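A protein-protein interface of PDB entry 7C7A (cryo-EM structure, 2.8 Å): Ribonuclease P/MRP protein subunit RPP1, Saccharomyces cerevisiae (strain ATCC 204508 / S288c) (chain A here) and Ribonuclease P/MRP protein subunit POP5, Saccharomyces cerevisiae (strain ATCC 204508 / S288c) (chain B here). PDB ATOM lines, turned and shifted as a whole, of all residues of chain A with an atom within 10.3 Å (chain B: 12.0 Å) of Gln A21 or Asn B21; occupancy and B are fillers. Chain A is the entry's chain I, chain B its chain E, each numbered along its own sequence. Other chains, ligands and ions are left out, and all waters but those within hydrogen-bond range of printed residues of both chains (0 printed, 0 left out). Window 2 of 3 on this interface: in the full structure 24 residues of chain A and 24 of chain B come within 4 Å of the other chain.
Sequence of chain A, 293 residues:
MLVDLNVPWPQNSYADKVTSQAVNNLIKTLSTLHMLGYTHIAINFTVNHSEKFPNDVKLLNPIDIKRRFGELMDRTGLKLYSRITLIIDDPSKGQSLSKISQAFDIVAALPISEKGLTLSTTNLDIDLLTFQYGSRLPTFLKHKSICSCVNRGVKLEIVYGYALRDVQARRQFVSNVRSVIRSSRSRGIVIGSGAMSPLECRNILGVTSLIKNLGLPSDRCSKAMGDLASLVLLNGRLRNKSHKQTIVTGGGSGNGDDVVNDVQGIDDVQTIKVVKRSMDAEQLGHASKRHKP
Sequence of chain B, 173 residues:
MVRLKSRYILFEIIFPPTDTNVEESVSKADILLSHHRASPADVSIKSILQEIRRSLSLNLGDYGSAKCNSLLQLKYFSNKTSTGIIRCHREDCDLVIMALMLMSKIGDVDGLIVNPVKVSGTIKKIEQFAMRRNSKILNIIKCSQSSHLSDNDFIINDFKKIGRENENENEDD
No residue of chain B comes within 4 Å of Thr A19.
No residue of chain B comes within 4 Å of Ser A20.
Gln A21 touches two residues of chain B.
No residue of chain B comes within 4 Å of Ala A22.
No residue of chain B comes within 4 Å of Val A23.
Printed residues of chain B within 4 Å of Asn A24: Thr B20 (3.3 Å).
No residue of chain B comes within 4 Å of Asn A25.
Arg A68 touches none of the printed residues of chain B.
Printed residues of chain A within 4 Å of Pro B16: Pro A198.
Of chain A, only Gln A21 (3.8 Å) comes within 4 Å of Asn B21.
No residue of chain A comes within 4 Å of Val B22.
Of the printed residues of chain A, Glu B24 touches Lys A28.
The nearest residue of chain B that does not touch Gln A21 is Asp B19 (7.4 Å).
The nearest printed residue of chain A that does not touch Pro B17 is Pro A198 (5.5 Å).
The side-chain amino group (NZ) of Lys A28 sits at hydrogen-bond distance from the backbone carbonyl oxygen (O) of Pro B17, 2.6 Å away.
The side-chain amino group of Lys A28 lies close to the backbone carbonyl oxygen of Asp B19, 3.4 Å away.
The side-chain hydroxyl of Thr B20 lies within hydrogen-bond range of the backbone carbonyl oxygen of Gln A21 (3.0 Å).
The backbone carbonyl oxygen (O) of Thr B20 lies within hydrogen-bond range of the side-chain amide nitrogen (ND2) of Asn A24, at 3.3 Å.
The side-chain carboxylate (OE2) of Glu B24 is in salt-bridge range of the side-chain amino group (NZ) of Lys A28, 3.5 Å away.
Among the printed residues, pairs that only touch across the chains: Pro A198 with Pro B16 (3.5 Å) and Gln A21 with Asn B21 (3.8 Å).
O of Ser A20 sits at hydrogen-bond distance from ND2 of Asn A24.
Printed residues of chain B that touch a printed residue of chain A: Pro B16, Pro B17, Asp B19, Thr B20, Asn B21 and Glu B24.
Of the 19 printed residues of chain A, 4 touch a printed residue of chain B.
Printed residues of chain A that touch a printed residue of chain B: Gln A21, Asn A24, Lys A28 and Pro A198.
Hydrophobic or aromatic side chains of chain A within 4 Å of the printed part of chain B: Pro A198.
Among the printed residues, 7 pairs touch across the chains.
Among the printed residues, Asp or Glu carboxylates within 4 Å of a Lys or Arg side-chain nitrogen of the other chain: Lys A28 with Glu B24 (3.5 Å).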
ATOM      1  N   TRP A   9       5.813   3.569  27.277  1.00  0.00           N
ATOM      2  CA  TRP A   9       6.001   4.977  27.611  1.00  0.00           C
ATOM      3  C   TRP A   9       6.521   5.102  29.038  1.00  0.00           C
ATOM      4  O   TRP A   9       5.987   4.446  29.943  1.00  0.00           O
ATOM      5  CB  TRP A   9       4.696   5.747  27.467  1.00  0.00           C
ATOM      6  CG  TRP A   9       4.839   7.229  27.640  1.00  0.00           C
ATOM      7  CD1 TRP A   9       4.846   7.920  28.816  1.00  0.00           C
ATOM      8  CD2 TRP A   9       4.989   8.206  26.602  1.00  0.00           C
ATOM      9  NE1 TRP A   9       4.994   9.265  28.576  1.00  0.00           N
ATOM     10  CE2 TRP A   9       5.084   9.466  27.224  1.00  0.00           C
ATOM     11  CE3 TRP A   9       5.054   8.136  25.207  1.00  0.00           C
ATOM     12  CZ2 TRP A   9       5.240  10.647  26.501  1.00  0.00           C
ATOM     13  CZ3 TRP A   9       5.208   9.309  24.490  1.00  0.00           C
ATOM     14  CH2 TRP A   9       5.300  10.547  25.138  1.00  0.00           C
ATOM     15  N   PRO A  10       7.548   5.917  29.283  1.00  0.00           N
ATOM     16  CA  PRO A  10       8.107   6.012  30.640  1.00  0.00           C
ATOM     17  C   PRO A  10       7.196   6.750  31.609  1.00  0.00           C
ATOM     18  O   PRO A  10       7.558   7.816  32.120  1.00  0.00           O
ATOM     19  CB  PRO A  10       9.427   6.771  30.427  1.00  0.00           C
ATOM     20  CG  PRO A  10       9.684   6.727  28.943  1.00  0.00           C
ATOM     21  CD  PRO A  10       8.335   6.687  28.308  1.00  0.00           C
ATOM     22  N   LYS A  17       4.850  13.447  36.303  1.00  0.00           N
ATOM     23  CA  LYS A  17       5.111  14.130  35.046  1.00  0.00           C
ATOM     24  C   LYS A  17       6.382  13.592  34.400  1.00  0.00           C
ATOM     25  O   LYS A  17       7.356  13.255  35.080  1.00  0.00           O
ATOM     26  CB  LYS A  17       5.232  15.639  35.271  1.00  0.00           C
ATOM     27  CG  LYS A  17       3.996  16.298  35.879  1.00  0.00           C
ATOM     28  CD  LYS A  17       2.846  16.402  34.883  1.00  0.00           C
ATOM     29  CE  LYS A  17       1.799  15.321  35.112  1.00  0.00           C
ATOM     30  NZ  LYS A  17       0.643  15.460  34.183  1.00  0.00           N
ATOM     31  N   VAL A  18       6.363  13.513  33.069  1.00  0.00           N
ATOM     32  CA  VAL A  18       7.502  12.970  32.340  1.00  0.00           C
ATOM     33  C   VAL A  18       8.628  13.997  32.292  1.00  0.00           C
ATOM     34  O   VAL A  18       8.405  15.211  32.402  1.00  0.00           O
ATOM     35  CB  VAL A  18       7.083  12.539  30.923  1.00  0.00           C
ATOM     36  CG1 VAL A  18       6.229  11.282  30.983  1.00  0.00           C
ATOM     37  CG2 VAL A  18       6.338  13.666  30.223  1.00  0.00           C
ATOM     38  N   THR A  19       9.851  13.504  32.129  1.00  0.00           N
ATOM     39  CA  THR A  19      11.040  14.339  32.063  1.00  0.00           C
ATOM     40  C   THR A  19      11.598  14.354  30.644  1.00  0.00           C
ATOM     41  O   THR A  19      11.202  13.561  29.786  1.00  0.00           O
ATOM     42  CB  THR A  19      12.115  13.849  33.040  1.00  0.00           C
ATOM     43  OG1 THR A  19      12.484  12.503  32.712  1.00  0.00           O
ATOM     44  CG2 THR A  19      11.596  13.893  34.469  1.00  0.00           C
ATOM     45  N   SER A  20      12.529  15.280  30.409  1.00  0.00           N
ATOM     46  CA  SER A  20      13.136  15.404  29.087  1.00  0.00           C
ATOM     47  C   SER A  20      14.014  14.200  28.769  1.00  0.00           C
ATOM     48  O   SER A  20      14.127  13.792  27.607  1.00  0.00           O
ATOM     49  CB  SER A  20      13.944  16.700  29.001  1.00  0.00           C
ATOM     50  OG  SER A  20      15.062  16.667  29.872  1.00  0.00           O
ATOM     51  N   GLN A  21      14.650  13.622  29.790  1.00  0.00           N
ATOM     52  CA  GLN A  21      15.530  12.478  29.568  1.00  0.00           C
ATOM     53  C   GLN A  21      14.747  11.263  29.086  1.00  0.00           C
ATOM     54  O   GLN A  21      15.213  10.509  28.224  1.00  0.00           O
ATOM     55  CB  GLN A  21      16.297  12.155  30.852  1.00  0.00           C
ATOM     56  CG  GLN A  21      17.238  13.261  31.301  1.00  0.00           C
ATOM     57  CD  GLN A  21      18.123  12.840  32.456  1.00  0.00           C
ATOM     58  OE1 GLN A  21      17.933  11.775  33.044  1.00  0.00           O
ATOM     59  NE2 GLN A  21      19.096  13.679  32.790  1.00  0.00           N
ATOM     60  N   ALA A  22      13.547  11.058  29.634  1.00  0.00           N
ATOM     61  CA  ALA A  22      12.719   9.941  29.193  1.00  0.00           C
ATOM     62  C   ALA A  22      12.283  10.118  27.743  1.00  0.00           C
ATOM     63  O   ALA A  22      12.291   9.158  26.962  1.00  0.00           O
ATOM     64  CB  ALA A  22      11.503   9.795  30.107  1.00  0.00           C
ATOM     65  N   VAL A  23      11.906  11.340  27.365  1.00  0.00           N
ATOM     66  CA  VAL A  23      11.527  11.605  25.981  1.00  0.00           C
ATOM     67  C   VAL A  23      12.720  11.408  25.055  1.00  0.00           C
ATOM     68  O   VAL A  23      12.584  10.875  23.947  1.00  0.00           O
ATOM     69  CB  VAL A  23      10.932  13.020  25.852  1.00  0.00           C
ATOM     70  CG1 VAL A  23      10.549  13.311  24.407  1.00  0.00           C
ATOM     71  CG2 VAL A  23       9.729  13.175  26.769  1.00  0.00           C
ATOM     72  N   ASN A  24      13.911  11.820  25.498  1.00  0.00           N
ATOM     73  CA  ASN A  24      15.108  11.622  24.687  1.00  0.00           C
ATOM     74  C   ASN A  24      15.418  10.141  24.510  1.00  0.00           C
ATOM     75  O   ASN A  24      15.786   9.706  23.413  1.00  0.00           O
ATOM     76  CB  ASN A  24      16.296  12.349  25.318  1.00  0.00           C
ATOM     77  CG  ASN A  24      16.231  13.851  25.122  1.00  0.00           C
ATOM     78  OD1 ASN A  24      15.748  14.334  24.099  1.00  0.00           O
ATOM     79  ND2 ASN A  24      16.719  14.598  26.106  1.00  0.00           N
ATOM     80  N   ASN A  25      15.268   9.349  25.574  1.00  0.00           N
ATOM     81  CA  ASN A  25      15.508   7.914  25.463  1.00  0.00           C
ATOM     82  C   ASN A  25      14.477   7.251  24.555  1.00  0.00           C
ATOM     83  O   ASN A  25      14.808   6.336  23.793  1.00  0.00           O
ATOM     84  CB  ASN A  25      15.499   7.270  26.849  1.00  0.00           C
ATOM     85  CG  ASN A  25      16.064   5.862  26.841  1.00  0.00           C
ATOM     86  OD1 ASN A  25      16.776   5.473  25.916  1.00  0.00           O
ATOM     87  ND2 ASN A  25      15.750   5.092  27.876  1.00  0.00           N
ATOM     88  N   LEU A  26      13.223   7.706  24.618  1.00  0.00           N
ATOM     89  CA  LEU A  26      12.204   7.177  23.717  1.00  0.00           C
ATOM     90  C   LEU A  26      12.513   7.533  22.268  1.00  0.00           C
ATOM     91  O   LEU A  26      12.302   6.716  21.362  1.00  0.00           O
ATOM     92  CB  LEU A  26      10.826   7.700  24.119  1.00  0.00           C
ATOM     93  CG  LEU A  26       9.639   7.151  23.326  1.00  0.00           C
ATOM     94  CD1 LEU A  26       9.531   5.645  23.502  1.00  0.00           C
ATOM     95  CD2 LEU A  26       8.352   7.835  23.749  1.00  0.00           C
ATOM     96  N   ILE A  27      13.013   8.748  22.030  1.00  0.00           N
ATOM     97  CA  ILE A  27      13.413   9.139  20.680  1.00  0.00           C
ATOM     98  C   ILE A  27      14.570   8.273  20.198  1.00  0.00           C
ATOM     99  O   ILE A  27      14.602   7.842  19.039  1.00  0.00           O
ATOM    100  CB  ILE A  27      13.767  10.638  20.640  1.00  0.00           C
ATOM    101  CG1 ILE A  27      12.504  11.488  20.796  1.00  0.00           C
ATOM    102  CG2 ILE A  27      14.492  10.989  19.349  1.00  0.00           C
ATOM    103  CD1 ILE A  27      12.760  12.979  20.746  1.00  0.00           C
ATOM    104  N   LYS A  28      15.537   8.006  21.080  1.00  0.00           N
ATOM    105  CA  LYS A  28      16.640   7.110  20.739  1.00  0.00           C
ATOM    106  C   LYS A  28      16.125   5.731  20.351  1.00  0.00           C
ATOM    107  O   LYS A  28      16.556   5.149  19.348  1.00  0.00           O
ATOM    108  CB  LYS A  28      17.611   7.001  21.916  1.00  0.00           C
ATOM    109  CG  LYS A  28      18.296   8.297  22.299  1.00  0.00           C
ATOM    110  CD  LYS A  28      19.381   8.667  21.312  1.00  0.00           C
ATOM    111  CE  LYS A  28      20.140   9.894  21.781  1.00  0.00           C
ATOM    112  NZ  LYS A  28      21.518   9.930  21.223  1.00  0.00           N
ATOM    113  N   THR A  29      15.198   5.190  21.146  1.00  0.00           N
ATOM    114  CA  THR A  29      14.645   3.871  20.864  1.00  0.00           C
ATOM    115  C   THR A  29      13.887   3.836  19.542  1.00  0.00           C
ATOM    116  O   THR A  29      14.055   2.892  18.764  1.00  0.00           O
ATOM    117  CB  THR A  29      13.725   3.430  22.004  1.00  0.00           C
ATOM    118  OG1 THR A  29      14.467   3.386  23.230  1.00  0.00           O
ATOM    119  CG2 THR A  29      13.145   2.052  21.723  1.00  0.00           C
ATOM    120  N   ARG A  68       5.003  16.525  19.519  1.00  0.00           N
ATOM    121  CA  ARG A  68       6.277  15.914  19.877  1.00  0.00           C
ATOM    122  C   ARG A  68       6.863  15.092  18.734  1.00  0.00           C
ATOM    123  O   ARG A  68       7.985  15.354  18.289  1.00  0.00           O
ATOM    124  CB  ARG A  68       6.113  15.040  21.124  1.00  0.00           C
ATOM    125  CG  ARG A  68       5.734  15.811  22.377  1.00  0.00           C
ATOM    126  CD  ARG A  68       5.494  14.871  23.548  1.00  0.00           C
ATOM    127  NE  ARG A  68       5.939  15.444  24.815  1.00  0.00           N
ATOM    128  CZ  ARG A  68       5.123  15.948  25.734  1.00  0.00           C
ATOM    129  NH1 ARG A  68       5.615  16.448  26.859  1.00  0.00           N
ATOM    130  NH2 ARG A  68       3.813  15.950  25.530  1.00  0.00           N
ATOM    131  N   MET A 196      12.403  -0.245  26.318  1.00  0.00           N
ATOM    132  CA  MET A 196      12.475   1.200  26.468  1.00  0.00           C
ATOM    133  C   MET A 196      13.855   1.772  26.180  1.00  0.00           C
ATOM    134  O   MET A 196      13.987   2.996  26.079  1.00  0.00           O
ATOM    135  CB  MET A 196      12.056   1.617  27.886  1.00  0.00           C
ATOM    136  CG  MET A 196      13.067   1.260  28.965  1.00  0.00           C
ATOM    137  SD  MET A 196      12.996  -0.480  29.427  1.00  0.00           S
ATOM    138  CE  MET A 196      11.435  -0.525  30.301  1.00  0.00           C
ATOM    139  N   SER A 197      14.873   0.927  26.046  1.00  0.00           N
ATOM    140  CA  SER A 197      16.227   1.356  25.751  1.00  0.00           C
ATOM    141  C   SER A 197      16.650   0.843  24.379  1.00  0.00           C
ATOM    142  O   SER A 197      16.276  -0.267  23.986  1.00  0.00           O
ATOM    143  CB  SER A 197      17.213   0.849  26.812  1.00  0.00           C
ATOM    144  OG  SER A 197      18.554   1.052  26.403  1.00  0.00           O
ATOM    145  N   PRO A 198      17.425   1.628  23.625  1.00  0.00           N
ATOM    146  CA  PRO A 198      17.834   1.196  22.280  1.00  0.00           C
ATOM    147  C   PRO A 198      18.802   0.021  22.263  1.00  0.00           C
ATOM    148  O   PRO A 198      19.137  -0.462  21.176  1.00  0.00           O
ATOM    149  CB  PRO A 198      18.489   2.457  21.696  1.00  0.00           C
ATOM    150  CG  PRO A 198      18.935   3.234  22.887  1.00  0.00           C
ATOM    151  CD  PRO A 198      17.902   2.985  23.942  1.00  0.00           C
ATOM    152  N   PRO B  16      23.929   1.751  18.972  1.00  0.00           N
ATOM    153  CA  PRO B  16      22.904   2.763  19.214  1.00  0.00           C
ATOM    154  C   PRO B  16      23.481   3.936  19.982  1.00  0.00           C
ATOM    155  O   PRO B  16      24.195   3.751  20.984  1.00  0.00           O
ATOM    156  CB  PRO B  16      21.851   2.008  20.048  1.00  0.00           C
ATOM    157  CG  PRO B  16      22.171   0.552  19.872  1.00  0.00           C
ATOM    158  CD  PRO B  16      23.649   0.496  19.686  1.00  0.00           C
ATOM    159  N   PRO B  17      23.200   5.168  19.554  1.00  0.00           N
ATOM    160  CA  PRO B  17      23.740   6.363  20.242  1.00  0.00           C
ATOM    161  C   PRO B  17      23.077   6.611  21.595  1.00  0.00           C
ATOM    162  O   PRO B  17      22.299   7.540  21.801  1.00  0.00           O
ATOM    163  CB  PRO B  17      23.449   7.489  19.244  1.00  0.00           C
ATOM    164  CG  PRO B  17      23.012   6.818  17.964  1.00  0.00           C
ATOM    165  CD  PRO B  17      22.404   5.527  18.371  1.00  0.00           C
ATOM    166  N   THR B  18      23.403   5.756  22.562  1.00  0.00           N
ATOM    167  CA  THR B  18      22.808   5.829  23.896  1.00  0.00           C
ATOM    168  C   THR B  18      23.425   7.000  24.660  1.00  0.00           C
ATOM    169  O   THR B  18      24.415   6.868  25.382  1.00  0.00           O
ATOM    170  CB  THR B  18      22.967   4.496  24.628  1.00  0.00           C
ATOM    171  OG1 THR B  18      22.444   4.603  25.959  1.00  0.00           O
ATOM    172  CG2 THR B  18      24.422   4.007  24.645  1.00  0.00           C
ATOM    173  N   ASP B  19      22.819   8.176  24.493  1.00  0.00           N
ATOM    174  CA  ASP B  19      23.265   9.379  25.196  1.00  0.00           C
ATOM    175  C   ASP B  19      22.052  10.296  25.336  1.00  0.00           C
ATOM    176  O   ASP B  19      21.699  11.007  24.390  1.00  0.00           O
ATOM    177  CB  ASP B  19      24.405  10.060  24.453  1.00  0.00           C
ATOM    178  CG  ASP B  19      25.154  11.054  25.320  1.00  0.00           C
ATOM    179  OD1 ASP B  19      24.814  11.180  26.515  1.00  0.00           O
ATOM    180  OD2 ASP B  19      26.087  11.706  24.808  1.00  0.00           O
ATOM    181  N   THR B  20      21.430  10.279  26.513  1.00  0.00           N
ATOM    182  CA  THR B  20      20.218  11.051  26.748  1.00  0.00           C
ATOM    183  C   THR B  20      20.489  12.513  27.073  1.00  0.00           C
ATOM    184  O   THR B  20      19.550  13.318  27.068  1.00  0.00           O
ATOM    185  CB  THR B  20      19.402  10.425  27.885  1.00  0.00           C
ATOM    186  OG1 THR B  20      18.137  11.088  27.993  1.00  0.00           O
ATOM    187  CG2 THR B  20      20.145  10.547  29.208  1.00  0.00           C
ATOM    188  N   ASN B  21      21.740  12.874  27.359  1.00  0.00           N
ATOM    189  CA  ASN B  21      22.082  14.253  27.679  1.00  0.00           C
ATOM    190  C   ASN B  21      22.286  15.120  26.445  1.00  0.00           C
ATOM    191  O   ASN B  21      22.300  16.351  26.568  1.00  0.00           O
ATOM    192  CB  ASN B  21      23.351  14.298  28.539  1.00  0.00           C
ATOM    193  CG  ASN B  21      23.098  13.879  29.973  1.00  0.00           C
ATOM    194  OD1 ASN B  21      22.061  14.201  30.552  1.00  0.00           O
ATOM    195  ND2 ASN B  21      24.048  13.156  30.555  1.00  0.00           N
ATOM    196  N   VAL B  22      22.443  14.519  25.270  1.00  0.00           N
ATOM    197  CA  VAL B  22      22.735  15.249  24.042  1.00  0.00           C
ATOM    198  C   VAL B  22      21.536  15.149  23.109  1.00  0.00           C
ATOM    199  O   VAL B  22      20.921  14.084  22.978  1.00  0.00           O
ATOM    200  CB  VAL B  22      24.013  14.709  23.367  1.00  0.00           C
ATOM    201  CG1 VAL B  22      24.278  15.421  22.046  1.00  0.00           C
ATOM    202  CG2 VAL B  22      25.209  14.852  24.296  1.00  0.00           C
ATOM    203  N   GLU B  23      21.202  16.267  22.466  1.00  0.00           N
ATOM    204  CA  GLU B  23      20.139  16.291  21.474  1.00  0.00           C
ATOM    205  C   GLU B  23      20.685  15.825  20.123  1.00  0.00           C
ATOM    206  O   GLU B  23      21.864  16.003  19.801  1.00  0.00           O
ATOM    207  CB  GLU B  23      19.543  17.698  21.386  1.00  0.00           C
ATOM    208  CG  GLU B  23      18.216  17.821  20.647  1.00  0.00           C
ATOM    209  CD  GLU B  23      18.382  18.031  19.154  1.00  0.00           C
ATOM    210  OE1 GLU B  23      19.441  18.540  18.735  1.00  0.00           O
ATOM    211  OE2 GLU B  23      17.437  17.716  18.402  1.00  0.00           O
ATOM    212  N   GLU B  24      19.811  15.218  19.322  1.00  0.00           N
ATOM    213  CA  GLU B  24      20.223  14.566  18.088  1.00  0.00           C
ATOM    214  C   GLU B  24      19.397  15.063  16.911  1.00  0.00           C
ATOM    215  O   GLU B  24      18.270  15.540  17.072  1.00  0.00           O
ATOM    216  CB  GLU B  24      20.096  13.041  18.197  1.00  0.00           C
ATOM    217  CG  GLU B  24      21.037  12.405  19.209  1.00  0.00           C
ATOM    218  CD  GLU B  24      22.479  12.391  18.741  1.00  0.00           C
ATOM    219  OE1 GLU B  24      22.707  12.316  17.516  1.00  0.00           O
ATOM    220  OE2 GLU B  24      23.384  12.447  19.599  1.00  0.00           O
ATOM    221  N   SER B  25      19.968  14.919  15.719  1.00  0.00           N
ATOM    222  CA  SER B  25      19.324  15.317  14.476  1.00  0.00           C
ATOM    223  C   SER B  25      18.525  14.146  13.926  1.00  0.00           C
ATOM    224  O   SER B  25      19.015  13.012  13.880  1.00  0.00           O
ATOM    225  CB  SER B  25      20.355  15.782  13.445  1.00  0.00           C
ATOM    226  OG  SER B  25      19.731  16.156  12.228  1.00  0.00           O
ATOM    227  N   ARG B  37      29.045   4.442  12.897  1.00  0.00           N
ATOM    228  CA  ARG B  37      30.215   5.269  13.176  1.00  0.00           C
ATOM    229  C   ARG B  37      31.513   4.515  12.920  1.00  0.00           C
ATOM    230  O   ARG B  37      32.258   4.854  11.995  1.00  0.00           O
ATOM    231  CB  ARG B  37      30.188   5.762  14.625  1.00  0.00           C
ATOM    232  CG  ARG B  37      28.934   6.524  15.017  1.00  0.00           C
ATOM    233  CD  ARG B  37      28.860   6.692  16.527  1.00  0.00           C
ATOM    234  NE  ARG B  37      27.775   7.576  16.936  1.00  0.00           N
ATOM    235  CZ  ARG B  37      27.468   7.843  18.202  1.00  0.00           C
ATOM    236  NH1 ARG B  37      26.464   8.662  18.486  1.00  0.00           N
ATOM    237  NH2 ARG B  37      28.165   7.291  19.186  1.00  0.00           N
